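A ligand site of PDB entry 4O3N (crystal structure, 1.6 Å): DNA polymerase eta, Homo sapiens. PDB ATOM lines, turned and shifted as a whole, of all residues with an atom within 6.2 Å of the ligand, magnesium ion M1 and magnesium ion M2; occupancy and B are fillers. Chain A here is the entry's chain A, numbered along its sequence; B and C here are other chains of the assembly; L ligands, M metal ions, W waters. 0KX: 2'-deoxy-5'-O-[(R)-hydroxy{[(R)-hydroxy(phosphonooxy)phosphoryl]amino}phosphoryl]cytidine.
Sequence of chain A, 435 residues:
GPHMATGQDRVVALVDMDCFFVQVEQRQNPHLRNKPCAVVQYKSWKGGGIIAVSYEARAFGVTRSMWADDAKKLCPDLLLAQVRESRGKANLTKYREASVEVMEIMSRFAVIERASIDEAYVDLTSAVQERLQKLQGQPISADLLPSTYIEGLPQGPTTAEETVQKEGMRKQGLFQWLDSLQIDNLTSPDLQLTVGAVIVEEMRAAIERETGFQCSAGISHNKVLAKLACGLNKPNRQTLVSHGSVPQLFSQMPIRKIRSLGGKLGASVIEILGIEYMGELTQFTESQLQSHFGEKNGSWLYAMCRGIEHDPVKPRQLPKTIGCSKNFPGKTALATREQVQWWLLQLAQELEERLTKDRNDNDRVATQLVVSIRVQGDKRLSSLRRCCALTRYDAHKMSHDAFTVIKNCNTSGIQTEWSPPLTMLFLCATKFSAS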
ATOM      1  N   ASP A  16     -12.917 -29.721  30.798  1.00  0.00           N
ATOM      2  CA  ASP A  16     -12.949 -28.429  30.091  1.00  0.00           C
ATOM      3  C   ASP A  16     -14.263 -27.748  30.367  1.00  0.00           C
ATOM      4  O   ASP A  16     -15.325 -28.305  30.105  1.00  0.00           O
ATOM      5  CB  ASP A  16     -12.776 -28.591  28.582  1.00  0.00           C
ATOM      6  CG  ASP A  16     -12.704 -27.274  27.885  1.00  0.00           C
ATOM      7  OD1 ASP A  16     -11.601 -26.813  27.645  1.00  0.00           O
ATOM      8  OD2 ASP A  16     -13.743 -26.709  27.649  1.00  0.00           O
ATOM      9  N   MET A  17     -14.202 -26.524  30.834  1.00  0.00           N
ATOM     10  CA  MET A  17     -15.442 -25.878  31.175  1.00  0.00           C
ATOM     11  C   MET A  17     -16.314 -25.546  29.954  1.00  0.00           C
ATOM     12  O   MET A  17     -15.813 -25.219  28.910  1.00  0.00           O
ATOM     13  CB  MET A  17     -15.174 -24.546  31.911  1.00  0.00           C
ATOM     14  CG  MET A  17     -14.269 -24.736  33.171  1.00  0.00           C
ATOM     15  SD  MET A  17     -14.831 -25.916  34.398  1.00  0.00           S
ATOM     16  CE  MET A  17     -16.319 -25.213  34.903  1.00  0.00           C
ATOM     17  N   ASP A  18     -17.608 -25.661  30.135  1.00  0.00           N
ATOM     18  CA  ASP A  18     -18.534 -25.325  29.034  1.00  0.00           C
ATOM     19  C   ASP A  18     -18.647 -23.800  28.926  1.00  0.00           C
ATOM     20  O   ASP A  18     -18.786 -23.126  29.959  1.00  0.00           O
ATOM     21  CB  ASP A  18     -19.891 -25.984  29.227  1.00  0.00           C
ATOM     22  CG  ASP A  18     -19.807 -27.526  29.254  1.00  0.00           C
ATOM     23  OD1 ASP A  18     -18.909 -28.100  28.615  1.00  0.00           O
ATOM     24  OD2 ASP A  18     -20.649 -28.135  29.875  1.00  0.00           O
ATOM     25  N   CYS A  19     -18.582 -23.306  27.693  1.00  0.00           N
ATOM     26  CA  CYS A  19     -18.684 -21.868  27.338  1.00  0.00           C
ATOM     27  C   CYS A  19     -18.250 -21.007  28.523  1.00  0.00           C
ATOM     28  O   CYS A  19     -19.033 -20.238  29.077  1.00  0.00           O
ATOM     29  CB  CYS A  19     -20.094 -21.486  26.854  1.00  0.00           C
ATOM     30  SG  CYS A  19     -21.519 -21.943  27.875  1.00  0.00           S
ATOM     31  N   PHE A  20     -16.974 -21.137  28.894  1.00  0.00           N
ATOM     32  CA  PHE A  20     -16.567 -20.736  30.248  1.00  0.00           C
ATOM     33  C   PHE A  20     -16.864 -19.270  30.574  1.00  0.00           C
ATOM     34  O   PHE A  20     -17.488 -19.025  31.579  1.00  0.00           O
ATOM     35  CB  PHE A  20     -15.087 -20.995  30.432  1.00  0.00           C
ATOM     36  CG  PHE A  20     -14.593 -20.746  31.831  1.00  0.00           C
ATOM     37  CD1 PHE A  20     -15.331 -21.149  32.940  1.00  0.00           C
ATOM     38  CD2 PHE A  20     -13.422 -20.033  32.034  1.00  0.00           C
ATOM     39  CE1 PHE A  20     -14.878 -20.925  34.240  1.00  0.00           C
ATOM     40  CE2 PHE A  20     -12.955 -19.795  33.376  1.00  0.00           C
ATOM     41  CZ  PHE A  20     -13.708 -20.239  34.429  1.00  0.00           C
ATOM     42  N   PHE A  21     -16.393 -18.324  29.755  1.00  0.00           N
ATOM     43  CA  PHE A  21     -16.563 -16.916  30.154  1.00  0.00           C
ATOM     44  C   PHE A  21     -18.049 -16.560  30.176  1.00  0.00           C
ATOM     45  O   PHE A  21     -18.461 -15.806  31.023  1.00  0.00           O
ATOM     46  CB  PHE A  21     -15.861 -15.918  29.234  1.00  0.00           C
ATOM     47  CG  PHE A  21     -14.370 -15.932  29.305  1.00  0.00           C
ATOM     48  CD1 PHE A  21     -13.662 -16.952  29.963  1.00  0.00           C
ATOM     49  CD2 PHE A  21     -13.663 -14.932  28.650  1.00  0.00           C
ATOM     50  CE1 PHE A  21     -12.247 -16.910  30.011  1.00  0.00           C
ATOM     51  CE2 PHE A  21     -12.257 -14.855  28.720  1.00  0.00           C
ATOM     52  CZ  PHE A  21     -11.553 -15.910  29.391  1.00  0.00           C
ATOM     53  N   VAL A  22     -18.858 -17.173  29.312  1.00  0.00           N
ATOM     54  CA  VAL A  22     -20.309 -16.967  29.381  1.00  0.00           C
ATOM     55  C   VAL A  22     -20.836 -17.484  30.734  1.00  0.00           C
ATOM     56  O   VAL A  22     -21.645 -16.810  31.364  1.00  0.00           O
ATOM     57  CB  VAL A  22     -20.988 -17.635  28.217  1.00  0.00           C
ATOM     58  CG1 VAL A  22     -22.524 -17.759  28.436  1.00  0.00           C
ATOM     59  CG2 VAL A  22     -20.675 -16.889  26.928  1.00  0.00           C
ATOM     60  N   ILE A  51     -15.764 -13.292  22.220  1.00  0.00           N
ATOM     61  CA  ILE A  51     -14.711 -14.260  22.635  1.00  0.00           C
ATOM     62  C   ILE A  51     -15.321 -15.507  23.305  1.00  0.00           C
ATOM     63  O   ILE A  51     -14.603 -16.493  23.511  1.00  0.00           O
ATOM     64  CB  ILE A  51     -13.692 -13.640  23.539  1.00  0.00           C
ATOM     65  CG1 ILE A  51     -14.268 -13.219  24.893  1.00  0.00           C
ATOM     66  CG2 ILE A  51     -12.959 -12.494  22.762  1.00  0.00           C
ATOM     67  CD1 ILE A  51     -13.209 -12.648  25.811  1.00  0.00           C
ATOM     68  N   ALA A  52     -16.624 -15.528  23.568  1.00  0.00           N
ATOM     69  CA  ALA A  52     -17.268 -16.759  24.099  1.00  0.00           C
ATOM     70  C   ALA A  52     -18.738 -16.710  23.798  1.00  0.00           C
ATOM     71  O   ALA A  52     -19.319 -15.610  23.789  1.00  0.00           O
ATOM     72  CB  ALA A  52     -17.023 -16.898  25.645  1.00  0.00           C
ATOM     73  N   VAL A  53     -19.362 -17.894  23.602  1.00  0.00           N
ATOM     74  CA  VAL A  53     -20.700 -17.987  23.067  1.00  0.00           C
ATOM     75  C   VAL A  53     -21.477 -19.065  23.783  1.00  0.00           C
ATOM     76  O   VAL A  53     -21.006 -20.232  23.821  1.00  0.00           O
ATOM     77  CB  VAL A  53     -20.644 -18.320  21.531  1.00  0.00           C
ATOM     78  CG1 VAL A  53     -22.037 -18.170  20.897  1.00  0.00           C
ATOM     79  CG2 VAL A  53     -19.670 -17.390  20.836  1.00  0.00           C
ATOM     80  N   TYR A  55     -24.360 -21.998  24.363  1.00  0.00           N
ATOM     81  CA  TYR A  55     -24.860 -22.986  23.410  1.00  0.00           C
ATOM     82  C   TYR A  55     -26.152 -22.555  22.761  1.00  0.00           C
ATOM     83  O   TYR A  55     -26.295 -22.844  21.566  1.00  0.00           O
ATOM     84  CB  TYR A  55     -24.974 -24.388  24.080  1.00  0.00           C
ATOM     85  CG  TYR A  55     -23.609 -25.020  24.218  1.00  0.00           C
ATOM     86  CD1 TYR A  55     -22.749 -24.644  25.248  1.00  0.00           C
ATOM     87  CD2 TYR A  55     -23.115 -25.876  23.244  1.00  0.00           C
ATOM     88  CE1 TYR A  55     -21.449 -25.145  25.309  1.00  0.00           C
ATOM     89  CE2 TYR A  55     -21.820 -26.373  23.283  1.00  0.00           C
ATOM     90  CZ  TYR A  55     -20.984 -26.033  24.317  1.00  0.00           C
ATOM     91  OH  TYR A  55     -19.704 -26.561  24.391  1.00  0.00           O
ATOM     92  N   ARG A  58     -24.939 -20.459  19.891  1.00  0.00           N
ATOM     93  CA  ARG A  58     -24.281 -21.280  18.842  1.00  0.00           C
ATOM     94  C   ARG A  58     -25.314 -21.860  17.851  1.00  0.00           C
ATOM     95  O   ARG A  58     -24.961 -22.035  16.659  1.00  0.00           O
ATOM     96  CB  ARG A  58     -23.462 -22.426  19.451  1.00  0.00           C
ATOM     97  CG  ARG A  58     -22.346 -21.921  20.292  1.00  0.00           C
ATOM     98  CD  ARG A  58     -21.515 -23.056  20.906  1.00  0.00           C
ATOM     99  NE  ARG A  58     -20.717 -22.525  22.027  1.00  0.00           N
ATOM    100  CZ  ARG A  58     -19.675 -23.130  22.576  1.00  0.00           C
ATOM    101  NH1 ARG A  58     -19.274 -24.319  22.117  1.00  0.00           N
ATOM    102  NH2 ARG A  58     -19.040 -22.521  23.603  1.00  0.00           N
ATOM    103  N   ARG A  64     -17.150 -17.479  18.077  1.00  0.00           N
ATOM    104  CA  ARG A  64     -16.017 -16.665  18.447  1.00  0.00           C
ATOM    105  C   ARG A  64     -15.420 -15.971  17.235  1.00  0.00           C
ATOM    106  O   ARG A  64     -15.489 -16.478  16.089  1.00  0.00           O
ATOM    107  CB  ARG A  64     -14.966 -17.517  19.170  1.00  0.00           C
ATOM    108  CG  ARG A  64     -13.725 -16.838  19.570  1.00  0.00           C
ATOM    109  CD  ARG A  64     -12.669 -17.898  19.846  1.00  0.00           C
ATOM    110  NE  ARG A  64     -13.165 -18.885  20.784  1.00  0.00           N
ATOM    111  CZ  ARG A  64     -13.205 -20.203  20.560  1.00  0.00           C
ATOM    112  NH1 ARG A  64     -12.781 -20.741  19.417  1.00  0.00           N
ATOM    113  NH2 ARG A  64     -13.662 -20.996  21.536  1.00  0.00           N
ATOM    114  N   LEU A  92      -8.811  -9.348  32.178  1.00  0.00           N
ATOM    115  CA  LEU A  92      -9.408 -10.693  32.291  1.00  0.00           C
ATOM    116  C   LEU A  92      -9.443 -11.249  33.724  1.00  0.00           C
ATOM    117  O   LEU A  92      -9.697 -12.451  33.923  1.00  0.00           O
ATOM    118  CB  LEU A  92      -8.641 -11.638  31.361  1.00  0.00           C
ATOM    119  CG  LEU A  92      -8.686 -11.217  29.915  1.00  0.00           C
ATOM    120  CD1 LEU A  92      -7.754 -12.148  29.227  1.00  0.00           C
ATOM    121  CD2 LEU A  92     -10.150 -11.357  29.398  1.00  0.00           C
ATOM    122  N   SER A 116      -5.100 -24.576  30.348  1.00  0.00           N
ATOM    123  CA  SER A 116      -5.581 -23.285  29.856  1.00  0.00           C
ATOM    124  C   SER A 116      -6.352 -22.628  30.992  1.00  0.00           C
ATOM    125  O   SER A 116      -6.507 -23.192  32.058  1.00  0.00           O
ATOM    126  CB  SER A 116      -6.519 -23.437  28.653  1.00  0.00           C
ATOM    127  OG  SER A 116      -7.857 -23.869  29.044  1.00  0.00           O
ATOM    128  N   ILE A 117      -6.967 -21.471  30.708  1.00  0.00           N
ATOM    129  CA  ILE A 117      -7.780 -20.842  31.758  1.00  0.00           C
ATOM    130  C   ILE A 117      -8.997 -21.708  32.179  1.00  0.00           C
ATOM    131  O   ILE A 117      -9.531 -21.544  33.283  1.00  0.00           O
ATOM    132  CB  ILE A 117      -8.224 -19.428  31.301  1.00  0.00           C
ATOM    133  CG1 ILE A 117      -8.660 -18.589  32.482  1.00  0.00           C
ATOM    134  CG2 ILE A 117      -9.341 -19.526  30.231  1.00  0.00           C
ATOM    135  CD1 ILE A 117      -8.769 -17.098  32.072  1.00  0.00           C
ATOM    136  N   ASP A 118      -9.415 -22.622  31.282  1.00  0.00           N
ATOM    137  CA  ASP A 118     -10.628 -23.358  31.596  1.00  0.00           C
ATOM    138  C   ASP A 118     -10.478 -24.868  31.485  1.00  0.00           C
ATOM    139  O   ASP A 118     -11.489 -25.565  31.464  1.00  0.00           O
ATOM    140  CB  ASP A 118     -11.820 -22.865  30.747  1.00  0.00           C
ATOM    141  CG  ASP A 118     -11.971 -23.632  29.410  1.00  0.00           C
ATOM    142  OD1 ASP A 118     -10.943 -23.969  28.742  1.00  0.00           O
ATOM    143  OD2 ASP A 118     -13.141 -24.004  29.124  1.00  0.00           O
ATOM    144  N   GLU A 119      -9.246 -25.373  31.471  1.00  0.00           N
ATOM    145  CA  GLU A 119      -9.110 -26.836  31.465  1.00  0.00           C
ATOM    146  C   GLU A 119      -7.882 -27.331  32.120  1.00  0.00           C
ATOM    147  O   GLU A 119      -6.877 -26.598  32.252  1.00  0.00           O
ATOM    148  CB  GLU A 119      -9.160 -27.398  30.080  1.00  0.00           C
ATOM    149  CG  GLU A 119      -7.999 -27.088  29.229  1.00  0.00           C
ATOM    150  CD  GLU A 119      -8.405 -26.965  27.772  1.00  0.00           C
ATOM    151  OE1 GLU A 119      -8.962 -25.922  27.393  1.00  0.00           O
ATOM    152  OE2 GLU A 119      -8.205 -27.924  26.982  1.00  0.00           O
ATOM    153  N   LYS A 227      -8.428 -35.366  25.620  1.00  0.00           N
ATOM    154  CA  LYS A 227      -8.856 -34.098  25.084  1.00  0.00           C
ATOM    155  C   LYS A 227      -9.852 -34.316  23.946  1.00  0.00           C
ATOM    156  O   LYS A 227     -10.879 -33.655  23.889  1.00  0.00           O
ATOM    157  CB  LYS A 227      -7.647 -33.273  24.564  1.00  0.00           C
ATOM    158  CG  LYS A 227      -8.017 -31.962  23.884  1.00  0.00           C
ATOM    159  CD  LYS A 227      -8.759 -30.995  24.872  1.00  0.00           C
ATOM    160  CE  LYS A 227      -8.817 -29.562  24.213  1.00  0.00           C
ATOM    161  NZ  LYS A 227      -9.741 -28.508  24.778  1.00  0.00           N
ATOM    162  N   LYS A 234     -19.703 -32.702  24.448  1.00  0.00           N
ATOM    163  CA  LYS A 234     -19.899 -31.406  25.087  1.00  0.00           C
ATOM    164  C   LYS A 234     -21.251 -30.866  24.598  1.00  0.00           C
ATOM    165  O   LYS A 234     -21.552 -31.033  23.388  1.00  0.00           O
ATOM    166  CB  LYS A 234     -18.726 -30.513  24.654  1.00  0.00           C
ATOM    167  CG  LYS A 234     -18.236 -29.504  25.553  1.00  0.00           C
ATOM    168  CD  LYS A 234     -17.037 -28.827  24.988  1.00  0.00           C
ATOM    169  CE  LYS A 234     -15.992 -28.679  26.106  1.00  0.00           C
ATOM    170  NZ  LYS A 234     -16.483 -27.784  27.273  1.00  0.00           N
ATOM    171  N   PRO A 235     -22.045 -30.155  25.437  1.00  0.00           N
ATOM    172  CA  PRO A 235     -21.702 -29.717  26.807  1.00  0.00           C
ATOM    173  C   PRO A 235     -22.311 -30.622  27.893  1.00  0.00           C
ATOM    174  O   PRO A 235     -23.249 -31.425  27.663  1.00  0.00           O
ATOM    175  CB  PRO A 235     -22.333 -28.317  26.905  1.00  0.00           C
ATOM    176  CG  PRO A 235     -23.690 -28.494  26.134  1.00  0.00           C
ATOM    177  CD  PRO A 235     -23.307 -29.517  24.989  1.00  0.00           C
ATOM    178  P    DT B   8      -7.276 -25.463  21.520  1.00  0.00           P
ATOM    179  OP1  DT B   8      -7.973 -26.720  21.900  1.00  0.00           O
ATOM    180  OP2  DT B   8      -7.617 -24.686  20.292  1.00  0.00           O
ATOM    181  O5'  DT B   8      -7.389 -24.444  22.744  1.00  0.00           O
ATOM    182  C5'  DT B   8      -7.128 -24.867  24.045  1.00  0.00           C
ATOM    183  C4'  DT B   8      -7.455 -23.725  24.939  1.00  0.00           C
ATOM    184  O4'  DT B   8      -6.724 -22.592  24.445  1.00  0.00           O
ATOM    185  C3'  DT B   8      -8.940 -23.339  24.925  1.00  0.00           C
ATOM    186  O3'  DT B   8      -9.393 -23.189  26.284  1.00  0.00           O
ATOM    187  C2'  DT B   8      -8.969 -22.026  24.129  1.00  0.00           C
ATOM    188  C1'  DT B   8      -7.586 -21.469  24.353  1.00  0.00           C
ATOM    189  N1   DT B   8      -7.100 -20.627  23.231  1.00  0.00           N
ATOM    190  C2   DT B   8      -6.804 -19.301  23.470  1.00  0.00           C
ATOM    191  O2   DT B   8      -6.966 -18.779  24.557  1.00  0.00           O
ATOM    192  N3   DT B   8      -6.331 -18.615  22.381  1.00  0.00           N
ATOM    193  C4   DT B   8      -6.160 -19.114  21.109  1.00  0.00           C
ATOM    194  O4   DT B   8      -5.745 -18.434  20.181  1.00  0.00           O
ATOM    195  C5   DT B   8      -6.514 -20.494  20.924  1.00  0.00           C
ATOM    196  C7   DT B   8      -6.344 -21.134  19.588  1.00  0.00           C
ATOM    197  C6   DT B   8      -6.955 -21.179  21.987  1.00  0.00           C
ATOM    198  P    DT C   3      -9.896  -8.585  11.078  1.00  0.00           P
ATOM    199  OP1  DT C   3      -8.780  -8.789  10.122  1.00  0.00           O
ATOM    200  OP2  DT C   3     -11.324  -8.892  10.772  1.00  0.00           O
ATOM    201  O5'  DT C   3      -9.461  -9.410  12.355  1.00  0.00           O
ATOM    202  C5'  DT C   3     -10.430 -10.147  13.077  1.00  0.00           C
ATOM    203  C4'  DT C   3     -10.411  -9.660  14.491  1.00  0.00           C
ATOM    204  O4'  DT C   3     -11.154 -10.557  15.351  1.00  0.00           O
ATOM    205  C3'  DT C   3      -9.005  -9.575  15.112  1.00  0.00           C
ATOM    206  O3'  DT C   3      -8.722  -8.266  15.463  1.00  0.00           O
ATOM    207  C2'  DT C   3      -9.095 -10.442  16.366  1.00  0.00           C
ATOM    208  C1'  DT C   3     -10.579 -10.350  16.631  1.00  0.00           C
ATOM    209  N1   DT C   3     -11.053 -11.367  17.534  1.00  0.00           N
ATOM    210  C2   DT C   3     -11.718 -10.977  18.688  1.00  0.00           C
ATOM    211  O2   DT C   3     -11.985  -9.786  18.964  1.00  0.00           O
ATOM    212  N3   DT C   3     -12.073 -11.999  19.471  1.00  0.00           N
ATOM    213  C4   DT C   3     -11.819 -13.362  19.254  1.00  0.00           C
ATOM    214  O4   DT C   3     -12.188 -14.230  20.038  1.00  0.00           O
ATOM    215  C5   DT C   3     -11.099 -13.692  18.063  1.00  0.00           C
ATOM    216  C7   DT C   3     -10.777 -15.135  17.745  1.00  0.00           C
ATOM    217  C6   DT C   3     -10.747 -12.689  17.267  1.00  0.00           C
ATOM    218  P    DG C   4      -7.396  -7.974  16.296  1.00  0.00           P
ATOM    219  OP1  DG C   4      -7.160  -6.514  16.276  1.00  0.00           O
ATOM    220  OP2  DG C   4      -6.445  -9.074  16.037  1.00  0.00           O
ATOM    221  O5'  DG C   4      -7.795  -8.277  17.811  1.00  0.00           O
ATOM    222  C5'  DG C   4      -8.614  -7.418  18.530  1.00  0.00           C
ATOM    223  C4'  DG C   4      -8.415  -7.725  20.007  1.00  0.00           C
ATOM    224  O4'  DG C   4      -8.722  -9.129  20.319  1.00  0.00           O
ATOM    225  C3'  DG C   4      -7.011  -7.511  20.514  1.00  0.00           C
ATOM    226  O3'  DG C   4      -7.144  -7.042  21.855  1.00  0.00           O
ATOM    227  C2'  DG C   4      -6.387  -8.898  20.448  1.00  0.00           C
ATOM    228  C1'  DG C   4      -7.590  -9.762  20.870  1.00  0.00           C
ATOM    229  N9   DG C   4      -7.582 -11.088  20.313  1.00  0.00           N
ATOM    230  C8   DG C   4      -7.144 -11.545  19.103  1.00  0.00           C
ATOM    231  N7   DG C   4      -7.353 -12.840  18.926  1.00  0.00           N
ATOM    232  C5   DG C   4      -7.975 -13.233  20.123  1.00  0.00           C
ATOM    233  C6   DG C   4      -8.467 -14.480  20.520  1.00  0.00           C
ATOM    234  O6   DG C   4      -8.392 -15.566  19.920  1.00  0.00           O
ATOM    235  N1   DG C   4      -9.041 -14.415  21.800  1.00  0.00           N
ATOM    236  C2   DG C   4      -9.142 -13.281  22.578  1.00  0.00           C
ATOM    237  N2   DG C   4      -9.703 -13.423  23.815  1.00  0.00           N
ATOM    238  N3   DG C   4      -8.696 -12.087  22.199  1.00  0.00           N
ATOM    239  C4   DG C   4      -8.154 -12.153  20.945  1.00  0.00           C
ATOM    240  P    DA C   5      -5.918  -6.668  22.800  1.00  0.00           P
ATOM    241  OP1  DA C   5      -6.256  -5.424  23.470  1.00  0.00           O
ATOM    242  OP2  DA C   5      -4.662  -6.752  22.015  1.00  0.00           O
ATOM    243  O5'  DA C   5      -5.823  -7.907  23.820  1.00  0.00           O
ATOM    244  C5'  DA C   5      -6.824  -8.045  24.805  1.00  0.00           C
ATOM    245  C4'  DA C   5      -6.489  -9.213  25.694  1.00  0.00           C
ATOM    246  O4'  DA C   5      -6.638 -10.421  24.914  1.00  0.00           O
ATOM    247  C3'  DA C   5      -5.085  -9.222  26.269  1.00  0.00           C
ATOM    248  O3'  DA C   5      -5.150  -9.757  27.587  1.00  0.00           O
ATOM    249  C2'  DA C   5      -4.335 -10.201  25.337  1.00  0.00           C
ATOM    250  C1'  DA C   5      -5.476 -11.213  25.055  1.00  0.00           C
ATOM    251  N9   DA C   5      -5.317 -12.011  23.854  1.00  0.00           N
ATOM    252  C8   DA C   5      -4.802 -11.612  22.640  1.00  0.00           C
ATOM    253  N7   DA C   5      -4.746 -12.562  21.749  1.00  0.00           N
ATOM    254  C5   DA C   5      -5.315 -13.659  22.388  1.00  0.00           C
ATOM    255  C6   DA C   5      -5.480 -14.977  21.982  1.00  0.00           C
ATOM    256  N6   DA C   5      -5.156 -15.427  20.747  1.00  0.00           N
ATOM    257  N1   DA C   5      -6.028 -15.819  22.885  1.00  0.00           N
ATOM    258  C2   DA C   5      -6.316 -15.373  24.115  1.00  0.00           C
ATOM    259  N3   DA C   5      -6.170 -14.163  24.617  1.00  0.00           N
ATOM    260  C4   DA C   5      -5.630 -13.348  23.692  1.00  0.00           C
HETATM  261  PG  0KX L   1     -16.676 -24.904  25.069  1.00  0.00           P
HETATM  262  O1G 0KX L   1     -15.408 -25.345  25.749  1.00  0.00           O
HETATM  263  O2G 0KX L   1     -16.666 -25.239  23.557  1.00  0.00           O
HETATM  264  O3G 0KX L   1     -17.908 -25.353  25.746  1.00  0.00           O
HETATM  265  PB  0KX L   1     -15.531 -22.328  25.793  1.00  0.00           P
HETATM  266  O1B 0KX L   1     -15.182 -22.809  27.184  1.00  0.00           O
HETATM  267  O2B 0KX L   1     -16.068 -20.928  25.688  1.00  0.00           O
HETATM  268  O3B 0KX L   1     -16.654 -23.270  25.171  1.00  0.00           O
HETATM  269  PA  0KX L   1     -12.679 -22.929  25.177  1.00  0.00           P
HETATM  270  O1A 0KX L   1     -11.930 -23.081  23.865  1.00  0.00           O
HETATM  271  O2A 0KX L   1     -12.578 -24.037  26.128  1.00  0.00           O
HETATM  272  N3A 0KX L   1     -14.257 -22.521  24.726  1.00  0.00           N
HETATM  273  O5' 0KX L   1     -12.071 -21.596  25.796  1.00  0.00           O
HETATM  274  C5' 0KX L   1     -12.276 -21.221  27.172  1.00  0.00           C
HETATM  275  C4' 0KX L   1     -12.445 -19.778  27.331  1.00  0.00           C
HETATM  276  O4' 0KX L   1     -11.161 -19.100  26.826  1.00  0.00           O
HETATM  277  C3' 0KX L   1     -13.527 -19.088  26.476  1.00  0.00           C
HETATM  278  O3' 0KX L   1     -14.810 -19.108  27.196  1.00  0.00           O
HETATM  279  C2' 0KX L   1     -13.057 -17.787  26.281  1.00  0.00           C
HETATM  280  C1' 0KX L   1     -11.462 -17.936  26.205  1.00  0.00           C
HETATM  281  N1  0KX L   1     -10.994 -17.992  24.857  1.00  0.00           N
HETATM  282  C2  0KX L   1     -10.425 -16.806  24.328  1.00  0.00           C
HETATM  283  N3  0KX L   1      -9.892 -16.900  23.014  1.00  0.00           N
HETATM  284  C4  0KX L   1      -9.944 -18.070  22.277  1.00  0.00           C
HETATM  285  C5  0KX L   1     -10.479 -19.280  22.840  1.00  0.00           C
HETATM  286  C6  0KX L   1     -11.004 -19.195  24.159  1.00  0.00           C
HETATM  287  O2  0KX L   1     -10.449 -15.735  24.989  1.00  0.00           O
HETATM  288  N4  0KX L   1      -9.378 -18.060  20.985  1.00  0.00           N
HETATM  289 MG    MG M   1     -14.231 -24.717  27.449  1.00  0.00          MG
HETATM  290 MG    MG M   2     -10.786 -25.099  26.908  1.00  0.00          MG
HETATM  291  O   HOH W   1     -17.447 -20.021  23.632  1.00  0.00           O
HETATM  292  O   HOH W   2      -8.083 -17.920  26.907  1.00  0.00           O
HETATM  293  O   HOH W   3     -11.033 -25.924  24.938  1.00  0.00           O
HETATM  294  O   HOH W   4     -13.555 -26.880  24.388  1.00  0.00           O
HETATM  295  O   HOH W   5     -15.542 -23.536  21.833  1.00  0.00           O
HETATM  296  O   HOH W   6      -9.576 -14.219  26.811  1.00  0.00           O
HETATM  297  O   HOH W   7      -9.979 -20.557  19.556  1.00  0.00           O
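An oxygen (O3G) of the ligand sits at hydrogen-bond distance from the backbone NH of Cys 19.
O6 of DG 4 of chain C is in hydrogen-bond range of a nitrogen (N4) of the ligand.
NH1 of Arg 58 lies within salt-bridge range of O2G of the ligand.
The guanidinium group (NH2) of Arg 64 is in salt-bridge range of an oxygen (O1A) of the ligand, at 3.6 Å.
The backbone NH (N) of Phe 21 sits at hydrogen-bond distance from an oxygen (O3') of the ligand, at 3.1 Å.
The side-chain hydroxyl of Tyr 55 sits at hydrogen-bond distance from an oxygen (O3G) of the ligand (2.6 Å).
NZ of Lys 234 is in salt-bridge range of O3G of the ligand, at 3.2 Å.
An oxygen (O2B) of the ligand sits at hydrogen-bond distance from the backbone NH (N) of Phe 20, at 3.3 Å.
N4 of the ligand lies close to N3 of DT 8 of chain B, at 3.4 Å.
The guanidinium group of Arg 58 is in hydrogen-bond range of the backbone carbonyl oxygen of Val 53 (2.9 Å).
The backbone carbonyl oxygen (O) of Asp 16 lies within hydrogen-bond range of the side-chain amino group (NZ) of Lys 234, 3.1 Å away.
The side-chain carboxylate (OD1) of Asp 18 lies within salt-bridge range of the side-chain amino group (NZ) of Lys 234, 2.8 Å away.
O3' of DT 8 of chain B sits close to the side-chain hydroxyl (OG) of Ser 116 (3.2 Å).
N of Glu 119 is in hydrogen-bond range of OG of Ser 116 (3.2 Å).
OE2 of Glu 119 lies within salt-bridge range of NZ of Lys 227 (2.7 Å).
The guanidinium group (NH1) of Arg 58 sits at hydrogen-bond distance from the side-chain hydroxyl (OH) of Tyr 55 (3.2 Å).
The backbone NH (N) of Asp 118 sits at hydrogen-bond distance from the side-chain hydroxyl (OG) of Ser 116 (3.0 Å).
Merely in contact with the ligand: Asp 18, Ile 51, Ala 52 and Ile 117.
Hydrophobic or aromatic side chains within 4 Å of the ligand: Phe 20, Phe 21, Ala 52, Tyr 55 and Ile 117.
16 residues have an atom within 4 Å of the ligand: Asp 16, Met 17, Asp 18, Cys 19, Phe 20, Phe 21, Ile 51, Ala 52, Tyr 55, Arg 58, Arg 64, Ile 117, Asp 118, Lys 234, DT 8 of chain B and DG 4 of chain C.
The nearest printed residue that does not touch the ligand is DA 5 of chain C (4.01 Å).
Residues that only touch magnesium ion M1: Lys 234 (3.8 Å).
The nearest printed residue that does not touch magnesium ion M1 is Asp 18 (4.4 Å).
Merely in contact with magnesium ion M2: Ser 116.
Five residues have an atom within 4 Å of magnesium ion M2: Asp 16, Ser 116, Asp 118, Glu 119 and DT 8 of chain B.
Along chain A the residues within 4 Å of magnesium ion M2 span positions 16 to 119.
Magnesium ion M1 is bound by OD2 of Asp 16 (2.1 Å), OD2 of Asp 118 (2.1 Å), O1B of the ligand (2.1 Å), O1G of the ligand (2.2 Å), O of Met 17 (2.2 Å) and O2A of the ligand (2.2 Å).
Magnesium ion M1 has six donor atoms within binding distance.
Magnesium ion M2 is bound by the side-chain carboxylate (OD1) of Asp 16 (2.0 Å).
OE1 of Glu 119 is bound to magnesium ion M2 (2.1 Å).
Magnesium ion M2 is bound by water W3 (2.2 Å).
Magnesium ion M2 is bound by OD1 of Asp 118, 2.2 Å away.
O2A of the ligand binds magnesium ion M2, 2.2 Å away.
Magnesium ion M2 is bound by O3' of DT 8 of chain B (2.4 Å).
Water W3 lies within hydrogen-bond range of the side-chain amino group (NZ) of Lys 227 (2.9 Å) and an oxygen (O1A) of the ligand (3.2 Å).
Water W6 lies within hydrogen-bond range of an oxygen (O2) of the ligand (2.5 Å) and N2 of DG 4 of chain C (3.1 Å).
Water W1 lies within hydrogen-bond range of O2B of the ligand (2.6 Å), N of Val 53 (2.9 Å) and NH2 of Arg 58 (3.0 Å).
Water W5 lies within hydrogen-bond range of an oxygen (O2G) of the ligand (2.7 Å) and the guanidinium group of Arg 64 (3.2 Å).
Water W7 lies within hydrogen-bond range of the guanidinium group of Arg 64 (2.8 Å) and a nitrogen (N4) of the ligand (2.9 Å).
Water W2 bridges O2 of DT 8 of chain B (2.7 Å) and O4' of the ligand (3.3 Å).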
